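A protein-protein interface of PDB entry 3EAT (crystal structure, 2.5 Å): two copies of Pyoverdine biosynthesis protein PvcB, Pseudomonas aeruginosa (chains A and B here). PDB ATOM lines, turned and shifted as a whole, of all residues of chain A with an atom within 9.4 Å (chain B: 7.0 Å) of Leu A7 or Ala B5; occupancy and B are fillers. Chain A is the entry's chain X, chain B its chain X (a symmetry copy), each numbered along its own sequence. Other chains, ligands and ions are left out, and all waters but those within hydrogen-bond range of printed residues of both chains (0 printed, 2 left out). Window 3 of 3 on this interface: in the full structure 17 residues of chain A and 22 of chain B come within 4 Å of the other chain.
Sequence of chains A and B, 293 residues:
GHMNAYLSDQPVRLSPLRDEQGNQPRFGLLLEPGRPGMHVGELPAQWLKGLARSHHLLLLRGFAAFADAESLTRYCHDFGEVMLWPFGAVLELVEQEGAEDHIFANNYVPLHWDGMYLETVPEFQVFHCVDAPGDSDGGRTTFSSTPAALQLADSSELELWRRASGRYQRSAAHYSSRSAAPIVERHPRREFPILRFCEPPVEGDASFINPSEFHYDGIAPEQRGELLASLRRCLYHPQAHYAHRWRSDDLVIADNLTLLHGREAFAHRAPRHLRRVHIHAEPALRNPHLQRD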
ATOM      1  N   ASN A   4     -11.068  -1.033 -23.315  1.00  0.00           N
ATOM      2  CA  ASN A   4     -11.621  -2.219 -22.683  1.00  0.00           C
ATOM      3  C   ASN A   4     -12.896  -2.776 -23.330  1.00  0.00           C
ATOM      4  O   ASN A   4     -13.998  -2.275 -23.062  1.00  0.00           O
ATOM      5  CB  ASN A   4     -11.910  -1.901 -21.230  1.00  0.00           C
ATOM      6  CG  ASN A   4     -11.638  -3.064 -20.331  1.00  0.00           C
ATOM      7  OD1 ASN A   4     -11.907  -4.244 -20.682  1.00  0.00           O
ATOM      8  ND2 ASN A   4     -11.090  -2.755 -19.149  1.00  0.00           N
ATOM      9  N   ALA A   5     -12.766  -3.832 -24.130  1.00  0.00           N
ATOM     10  CA  ALA A   5     -13.890  -4.283 -24.948  1.00  0.00           C
ATOM     11  C   ALA A   5     -14.800  -5.412 -24.420  1.00  0.00           C
ATOM     12  O   ALA A   5     -15.683  -5.853 -25.143  1.00  0.00           O
ATOM     13  CB  ALA A   5     -13.404  -4.607 -26.377  1.00  0.00           C
ATOM     14  N   TYR A   6     -14.616  -5.880 -23.192  1.00  0.00           N
ATOM     15  CA  TYR A   6     -15.366  -7.056 -22.737  1.00  0.00           C
ATOM     16  C   TYR A   6     -16.354  -6.744 -21.647  1.00  0.00           C
ATOM     17  O   TYR A   6     -16.045  -6.003 -20.726  1.00  0.00           O
ATOM     18  CB  TYR A   6     -14.446  -8.144 -22.206  1.00  0.00           C
ATOM     19  CG  TYR A   6     -13.383  -8.580 -23.164  1.00  0.00           C
ATOM     20  CD1 TYR A   6     -13.693  -9.377 -24.270  1.00  0.00           C
ATOM     21  CD2 TYR A   6     -12.063  -8.187 -22.968  1.00  0.00           C
ATOM     22  CE1 TYR A   6     -12.685  -9.772 -25.166  1.00  0.00           C
ATOM     23  CE2 TYR A   6     -11.066  -8.561 -23.839  1.00  0.00           C
ATOM     24  CZ  TYR A   6     -11.371  -9.358 -24.932  1.00  0.00           C
ATOM     25  OH  TYR A   6     -10.348  -9.725 -25.784  1.00  0.00           O
ATOM     26  N   LEU A   7     -17.554  -7.298 -21.791  1.00  0.00           N
ATOM     27  CA  LEU A   7     -18.553  -7.347 -20.731  1.00  0.00           C
ATOM     28  C   LEU A   7     -19.083  -8.754 -20.721  1.00  0.00           C
ATOM     29  O   LEU A   7     -19.496  -9.285 -21.756  1.00  0.00           O
ATOM     30  CB  LEU A   7     -19.690  -6.371 -20.962  1.00  0.00           C
ATOM     31  CG  LEU A   7     -19.592  -5.015 -20.259  1.00  0.00           C
ATOM     32  CD1 LEU A   7     -20.969  -4.392 -20.285  1.00  0.00           C
ATOM     33  CD2 LEU A   7     -19.081  -5.108 -18.809  1.00  0.00           C
ATOM     34  N   SER A   8     -18.992  -9.383 -19.562  1.00  0.00           N
ATOM     35  CA  SER A   8     -19.399 -10.760 -19.432  1.00  0.00           C
ATOM     36  C   SER A   8     -20.833 -10.794 -18.943  1.00  0.00           C
ATOM     37  O   SER A   8     -21.336  -9.824 -18.359  1.00  0.00           O
ATOM     38  CB  SER A   8     -18.490 -11.464 -18.441  1.00  0.00           C
ATOM     39  OG  SER A   8     -18.476 -12.849 -18.683  1.00  0.00           O
ATOM     40  N   ASP A   9     -21.498 -11.902 -19.217  1.00  0.00           N
ATOM     41  CA  ASP A   9     -22.746 -12.216 -18.558  1.00  0.00           C
ATOM     42  C   ASP A   9     -22.461 -12.967 -17.237  1.00  0.00           C
ATOM     43  O   ASP A   9     -23.375 -13.200 -16.442  1.00  0.00           O
ATOM     44  CB  ASP A   9     -23.723 -12.953 -19.493  1.00  0.00           C
ATOM     45  CG  ASP A   9     -23.050 -14.031 -20.383  1.00  0.00           C
ATOM     46  OD1 ASP A   9     -21.845 -14.399 -20.189  1.00  0.00           O
ATOM     47  OD2 ASP A   9     -23.760 -14.518 -21.309  1.00  0.00           O
ATOM     48  N   GLN A  10     -21.189 -13.309 -17.008  1.00  0.00           N
ATOM     49  CA  GLN A  10     -20.713 -13.845 -15.734  1.00  0.00           C
ATOM     50  C   GLN A  10     -20.406 -12.730 -14.714  1.00  0.00           C
ATOM     51  O   GLN A  10     -20.122 -11.585 -15.099  1.00  0.00           O
ATOM     52  CB  GLN A  10     -19.448 -14.671 -15.956  1.00  0.00           C
ATOM     53  CG  GLN A  10     -19.601 -15.868 -16.880  1.00  0.00           C
ATOM     54  CD  GLN A  10     -20.520 -16.959 -16.335  1.00  0.00           C
ATOM     55  OE1 GLN A  10     -21.197 -17.643 -17.108  1.00  0.00           O
ATOM     56  NE2 GLN A  10     -20.529 -17.137 -15.021  1.00  0.00           N
ATOM     57  N   PRO A  11     -20.441 -13.056 -13.405  1.00  0.00           N
ATOM     58  CA  PRO A  11     -20.161 -12.041 -12.362  1.00  0.00           C
ATOM     59  C   PRO A  11     -18.651 -11.783 -12.205  1.00  0.00           C
ATOM     60  O   PRO A  11     -18.057 -12.086 -11.166  1.00  0.00           O
ATOM     61  CB  PRO A  11     -20.751 -12.674 -11.105  1.00  0.00           C
ATOM     62  CG  PRO A  11     -20.560 -14.186 -11.324  1.00  0.00           C
ATOM     63  CD  PRO A  11     -20.722 -14.389 -12.830  1.00  0.00           C
ATOM     64  N   VAL A  12     -18.034 -11.246 -13.257  1.00  0.00           N
ATOM     65  CA  VAL A  12     -16.597 -10.981 -13.278  1.00  0.00           C
ATOM     66  C   VAL A  12     -16.311  -9.688 -14.028  1.00  0.00           C
ATOM     67  O   VAL A  12     -17.144  -9.234 -14.801  1.00  0.00           O
ATOM     68  CB  VAL A  12     -15.807 -12.117 -13.980  1.00  0.00           C
ATOM     69  CG1 VAL A  12     -15.806 -13.329 -13.142  1.00  0.00           C
ATOM     70  CG2 VAL A  12     -16.420 -12.422 -15.325  1.00  0.00           C
ATOM     71  N   ARG A  13     -15.140  -9.097 -13.788  1.00  0.00           N
ATOM     72  CA  ARG A  13     -14.650  -7.999 -14.617  1.00  0.00           C
ATOM     73  C   ARG A  13     -13.575  -8.557 -15.516  1.00  0.00           C
ATOM     74  O   ARG A  13     -12.563  -9.094 -15.023  1.00  0.00           O
ATOM     75  CB  ARG A  13     -14.066  -6.867 -13.777  1.00  0.00           C
ATOM     76  CG  ARG A  13     -15.082  -5.923 -13.180  1.00  0.00           C
ATOM     77  CD  ARG A  13     -14.434  -5.077 -12.075  1.00  0.00           C
ATOM     78  NE  ARG A  13     -13.996  -5.881 -10.917  1.00  0.00           N
ATOM     79  CZ  ARG A  13     -12.786  -5.816 -10.356  1.00  0.00           C
ATOM     80  NH1 ARG A  13     -11.878  -4.961 -10.825  1.00  0.00           N
ATOM     81  NH2 ARG A  13     -12.492  -6.589  -9.306  1.00  0.00           N
ATOM     82  N   LEU A  14     -13.803  -8.443 -16.825  1.00  0.00           N
ATOM     83  CA  LEU A  14     -12.823  -8.869 -17.812  1.00  0.00           C
ATOM     84  C   LEU A  14     -12.081  -7.685 -18.410  1.00  0.00           C
ATOM     85  O   LEU A  14     -12.635  -6.598 -18.546  1.00  0.00           O
ATOM     86  CB  LEU A  14     -13.485  -9.671 -18.935  1.00  0.00           C
ATOM     87  CG  LEU A  14     -14.246 -10.938 -18.551  1.00  0.00           C
ATOM     88  CD1 LEU A  14     -14.524 -11.751 -19.769  1.00  0.00           C
ATOM     89  CD2 LEU A  14     -13.470 -11.770 -17.575  1.00  0.00           C
ATOM     90  N   SER A  15     -10.821  -7.901 -18.765  1.00  0.00           N
ATOM     91  CA  SER A  15     -10.065  -6.904 -19.522  1.00  0.00           C
ATOM     92  C   SER A  15      -8.873  -7.542 -20.192  1.00  0.00           C
ATOM     93  O   SER A  15      -8.470  -8.646 -19.808  1.00  0.00           O
ATOM     94  CB  SER A  15      -9.653  -5.699 -18.659  1.00  0.00           C
ATOM     95  OG  SER A  15      -9.194  -6.085 -17.396  1.00  0.00           O
ATOM     96  N   PRO A  16      -8.308  -6.864 -21.209  1.00  0.00           N
ATOM     97  CA  PRO A  16      -7.157  -7.439 -21.898  1.00  0.00           C
ATOM     98  C   PRO A  16      -5.979  -7.686 -20.957  1.00  0.00           C
ATOM     99  O   PRO A  16      -5.720  -6.901 -20.043  1.00  0.00           O
ATOM    100  CB  PRO A  16      -6.806  -6.372 -22.950  1.00  0.00           C
ATOM    101  CG  PRO A  16      -8.085  -5.606 -23.159  1.00  0.00           C
ATOM    102  CD  PRO A  16      -8.687  -5.553 -21.779  1.00  0.00           C
ATOM    103  N   LEU A  29      -6.149 -12.773 -21.244  1.00  0.00           N
ATOM    104  CA  LEU A  29      -7.325 -12.153 -20.682  1.00  0.00           C
ATOM    105  C   LEU A  29      -7.187 -12.084 -19.161  1.00  0.00           C
ATOM    106  O   LEU A  29      -6.736 -13.031 -18.533  1.00  0.00           O
ATOM    107  CB  LEU A  29      -8.582 -12.937 -21.080  1.00  0.00           C
ATOM    108  CG  LEU A  29      -9.928 -12.342 -20.650  1.00  0.00           C
ATOM    109  CD1 LEU A  29     -10.269 -11.070 -21.460  1.00  0.00           C
ATOM    110  CD2 LEU A  29     -11.019 -13.374 -20.783  1.00  0.00           C
ATOM    111  N   GLY A  34     -16.311 -10.282  -9.392  1.00  0.00           N
ATOM    112  CA  GLY A  34     -17.426  -9.352  -9.515  1.00  0.00           C
ATOM    113  C   GLY A  34     -18.187  -9.170  -8.216  1.00  0.00           C
ATOM    114  O   GLY A  34     -19.150  -8.385  -8.155  1.00  0.00           O
ATOM    115  N   TRP A  47     -17.131 -22.673 -18.910  1.00  0.00           N
ATOM    116  CA  TRP A  47     -16.969 -21.338 -19.434  1.00  0.00           C
ATOM    117  C   TRP A  47     -15.485 -20.924 -19.484  1.00  0.00           C
ATOM    118  O   TRP A  47     -15.013 -20.387 -20.495  1.00  0.00           O
ATOM    119  CB  TRP A  47     -17.793 -20.373 -18.593  1.00  0.00           C
ATOM    120  CG  TRP A  47     -17.643 -18.938 -18.980  1.00  0.00           C
ATOM    121  CD1 TRP A  47     -18.127 -18.354 -20.096  1.00  0.00           C
ATOM    122  CD2 TRP A  47     -16.972 -17.906 -18.243  1.00  0.00           C
ATOM    123  NE1 TRP A  47     -17.816 -17.021 -20.110  1.00  0.00           N
ATOM    124  CE2 TRP A  47     -17.106 -16.717 -18.983  1.00  0.00           C
ATOM    125  CE3 TRP A  47     -16.285 -17.871 -17.029  1.00  0.00           C
ATOM    126  CZ2 TRP A  47     -16.579 -15.492 -18.552  1.00  0.00           C
ATOM    127  CZ3 TRP A  47     -15.754 -16.645 -16.588  1.00  0.00           C
ATOM    128  CH2 TRP A  47     -15.906 -15.475 -17.353  1.00  0.00           C
ATOM    129  N   LEU A  51     -13.018 -19.750 -22.766  1.00  0.00           N
ATOM    130  CA  LEU A  51     -12.139 -18.575 -22.811  1.00  0.00           C
ATOM    131  C   LEU A  51     -10.672 -18.964 -22.958  1.00  0.00           C
ATOM    132  O   LEU A  51      -9.921 -18.320 -23.694  1.00  0.00           O
ATOM    133  CB  LEU A  51     -12.314 -17.732 -21.552  1.00  0.00           C
ATOM    134  CG  LEU A  51     -13.711 -17.165 -21.319  1.00  0.00           C
ATOM    135  CD1 LEU A  51     -13.697 -16.420 -20.009  1.00  0.00           C
ATOM    136  CD2 LEU A  51     -14.082 -16.254 -22.472  1.00  0.00           C
ATOM    137  N   MET B   3     -27.526   0.278 -11.257  1.00  0.00           N
ATOM    138  CA  MET B   3     -26.792   0.193 -12.537  1.00  0.00           C
ATOM    139  C   MET B   3     -26.911  -1.193 -13.213  1.00  0.00           C
ATOM    140  O   MET B   3     -27.141  -2.210 -12.559  1.00  0.00           O
ATOM    141  CB  MET B   3     -25.313   0.609 -12.385  1.00  0.00           C
ATOM    142  CG  MET B   3     -25.064   2.131 -12.230  1.00  0.00           C
ATOM    143  SD  MET B   3     -25.891   3.225 -13.445  1.00  0.00           S
ATOM    144  CE  MET B   3     -24.713   3.140 -14.788  1.00  0.00           C
ATOM    145  N   ASN B   4     -26.728  -1.226 -14.527  1.00  0.00           N
ATOM    146  CA  ASN B   4     -26.896  -2.455 -15.286  1.00  0.00           C
ATOM    147  C   ASN B   4     -25.654  -2.929 -16.053  1.00  0.00           C
ATOM    148  O   ASN B   4     -25.381  -2.435 -17.157  1.00  0.00           O
ATOM    149  CB  ASN B   4     -28.033  -2.264 -16.270  1.00  0.00           C
ATOM    150  CG  ASN B   4     -28.843  -3.508 -16.447  1.00  0.00           C
ATOM    151  OD1 ASN B   4     -28.304  -4.647 -16.470  1.00  0.00           O
ATOM    152  ND2 ASN B   4     -30.163  -3.316 -16.568  1.00  0.00           N
ATOM    153  N   ALA B   5     -24.938  -3.911 -15.512  1.00  0.00           N
ATOM    154  CA  ALA B   5     -23.633  -4.267 -16.065  1.00  0.00           C
ATOM    155  C   ALA B   5     -23.537  -5.422 -17.083  1.00  0.00           C
ATOM    156  O   ALA B   5     -22.434  -5.781 -17.476  1.00  0.00           O
ATOM    157  CB  ALA B   5     -22.614  -4.470 -14.923  1.00  0.00           C
ATOM    158  N   TYR B   6     -24.647  -6.002 -17.521  1.00  0.00           N
ATOM    159  CA  TYR B   6     -24.564  -7.202 -18.363  1.00  0.00           C
ATOM    160  C   TYR B   6     -25.040  -6.971 -19.771  1.00  0.00           C
ATOM    161  O   TYR B   6     -26.053  -6.322 -19.984  1.00  0.00           O
ATOM    162  CB  TYR B   6     -25.386  -8.348 -17.797  1.00  0.00           C
ATOM    163  CG  TYR B   6     -25.051  -8.715 -16.386  1.00  0.00           C
ATOM    164  CD1 TYR B   6     -23.873  -9.404 -16.080  1.00  0.00           C
ATOM    165  CD2 TYR B   6     -25.912  -8.365 -15.351  1.00  0.00           C
ATOM    166  CE1 TYR B   6     -23.569  -9.734 -14.749  1.00  0.00           C
ATOM    167  CE2 TYR B   6     -25.625  -8.676 -14.042  1.00  0.00           C
ATOM    168  CZ  TYR B   6     -24.462  -9.367 -13.738  1.00  0.00           C
ATOM    169  OH  TYR B   6     -24.204  -9.673 -12.417  1.00  0.00           O
ATOM    170  N   LEU B   7     -24.269  -7.489 -20.722  1.00  0.00           N
ATOM    171  CA  LEU B   7     -24.682  -7.615 -22.115  1.00  0.00           C
ATOM    172  C   LEU B   7     -24.304  -9.008 -22.537  1.00  0.00           C
ATOM    173  O   LEU B   7     -23.160  -9.437 -22.365  1.00  0.00           O
ATOM    174  CB  LEU B   7     -24.001  -6.603 -23.015  1.00  0.00           C
ATOM    175  CG  LEU B   7     -24.774  -5.317 -23.320  1.00  0.00           C
ATOM    176  CD1 LEU B   7     -24.119  -4.671 -24.519  1.00  0.00           C
ATOM    177  CD2 LEU B   7     -26.272  -5.550 -23.596  1.00  0.00           C
ATOM    178  N   SER B   8     -25.296  -9.741 -23.016  1.00  0.00           N
ATOM    179  CA  SER B   8     -25.085 -11.116 -23.393  1.00  0.00           C
ATOM    180  C   SER B   8     -24.790 -11.169 -24.879  1.00  0.00           C
ATOM    181  O   SER B   8     -25.126 -10.247 -25.634  1.00  0.00           O
ATOM    182  CB  SER B   8     -26.333 -11.922 -23.077  1.00  0.00           C
ATOM    183  OG  SER B   8     -26.010 -13.280 -22.903  1.00  0.00           O
ATOM    184  N   ASP B   9     -24.127 -12.236 -25.286  1.00  0.00           N
ATOM    185  CA  ASP B   9     -24.046 -12.587 -26.687  1.00  0.00           C
ATOM    186  C   ASP B   9     -25.262 -13.458 -27.075  1.00  0.00           C
ATOM    187  O   ASP B   9     -25.472 -13.746 -28.254  1.00  0.00           O
ATOM    188  CB  ASP B   9     -22.688 -13.219 -27.046  1.00  0.00           C
ATOM    189  CG  ASP B   9     -22.162 -14.225 -25.987  1.00  0.00           C
ATOM    190  OD1 ASP B   9     -22.898 -14.630 -25.029  1.00  0.00           O
ATOM    191  OD2 ASP B   9     -20.968 -14.613 -26.128  1.00  0.00           O
ATOM    192  N   LEU B  14     -30.323  -9.142 -19.908  1.00  0.00           N
ATOM    193  CA  LEU B  14     -29.923  -9.494 -18.555  1.00  0.00           C
ATOM    194  C   LEU B  14     -29.879  -8.275 -17.649  1.00  0.00           C
ATOM    195  O   LEU B  14     -29.581  -7.171 -18.094  1.00  0.00           O
ATOM    196  CB  LEU B  14     -28.555 -10.180 -18.547  1.00  0.00           C
ATOM    197  CG  LEU B  14     -28.398 -11.463 -19.359  1.00  0.00           C
ATOM    198  CD1 LEU B  14     -27.137 -12.159 -18.970  1.00  0.00           C
ATOM    199  CD2 LEU B  14     -29.553 -12.393 -19.148  1.00  0.00           C
ATOM    200  N   SER B  15     -30.182  -8.480 -16.373  1.00  0.00           N
ATOM    201  CA  SER B  15     -29.991  -7.432 -15.372  1.00  0.00           C
ATOM    202  C   SER B  15     -29.952  -8.028 -13.986  1.00  0.00           C
ATOM    203  O   SER B  15     -30.389  -9.169 -13.795  1.00  0.00           O
ATOM    204  CB  SER B  15     -31.046  -6.317 -15.479  1.00  0.00           C
ATOM    205  OG  SER B  15     -32.331  -6.823 -15.698  1.00  0.00           O
ATOM    206  N   PRO B  16     -29.416  -7.271 -13.010  1.00  0.00           N
ATOM    207  CA  PRO B  16     -29.344  -7.802 -11.652  1.00  0.00           C
ATOM    208  C   PRO B  16     -30.722  -8.153 -11.092  1.00  0.00           C
ATOM    209  O   PRO B  16     -31.708  -7.458 -11.346  1.00  0.00           O
ATOM    210  CB  PRO B  16     -28.704  -6.651 -10.856  1.00  0.00           C
ATOM    211  CG  PRO B  16     -27.953  -5.847 -11.883  1.00  0.00           C
ATOM    212  CD  PRO B  16     -28.849  -5.908 -13.093  1.00  0.00           C
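OG of Ser B8 is in hydrogen-bond range of OD2 of Asp A9 (3.0 Å).
N of Gln A10 sits close to OG of Ser A8 (3.2 Å).
The backbone carbonyl oxygen (O) of Leu B14 lies close to the side-chain amide oxygen (OD1) of Asn B4, at 3.3 Å.
CD1 of Leu A7 touches O of Ala B5, 3.5 Å away.
O of Leu A7 touches O of Leu B7, at 3.7 Å.
O of Ser A8 touches CD1 of Tyr B6, 3.4 Å away.
Asp A9 touches Tyr B6 (O to CD1, 3.8 Å).
Asp A9 touches Asp B9.
Leu B14 touches Asp A9.
Gln A10 touches Tyr B6 (O to CE1, 3.9 Å).
Leu A7 touches just these residues of chain B: Ala B5 and Leu B7.
Printed residues of chain B within 4 Å of Ser A8: Tyr B6.
Of the printed residues of chain B, Asp A9 touches Tyr B6 (3.8 Å), Ser B8 (3.0 Å), Asp B9 (3.8 Å) and Leu B14 (3.5 Å).
Trp A47 touches none of the printed residues of chain B.
Of the printed residues of chain A, Ala B5 touches Leu A7.
The nearest residue of chain B that does not touch Leu A7 is Tyr B6 (4.8 Å).
The nearest residue of chain A that does not touch Ala B5 is Ser A8 (4.3 Å).
Of the 17 printed residues of chain A, 4 touch a printed residue of chain B.
Hydrophobic or aromatic side chains of chain A that line the printed part of chain B: Leu A7.
Along chain A the printed residues that touch a printed residue of chain B span positions 7 to 10.
Printed residues of chain B that touch a printed residue of chain A: Ala B5, Tyr B6, Leu B7, Ser B8, Asp B9 and Leu B14.
Hydrophobic or aromatic side chains of chain B that line the printed part of chain A: Tyr B6 and Leu B14.
Among the printed residues, 8 pairs touch across the chains.
Among the printed residues, no Asp or Glu carboxylate lies within 4 Å of a Lys or Arg side-chain nitrogen of the other chain.
Leu A7 touches Ala B5, but with the chains exchanged Ala A5 does not touch Leu B7 (8.5 Å).
Asp A9 touches Tyr B6, but with the chains exchanged Tyr A6 does not touch Asp B9 (9.2 Å).
Asp A9 touches Ser B8, but with the chains exchanged Ser A8 does not touch Asp B9 (7.3 Å).
Asp B9 touches its own counterpart, Asp A9.
Positions printed for both chains: 4, 5, 6, 7, 8, 9, 14, 15 and 16.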
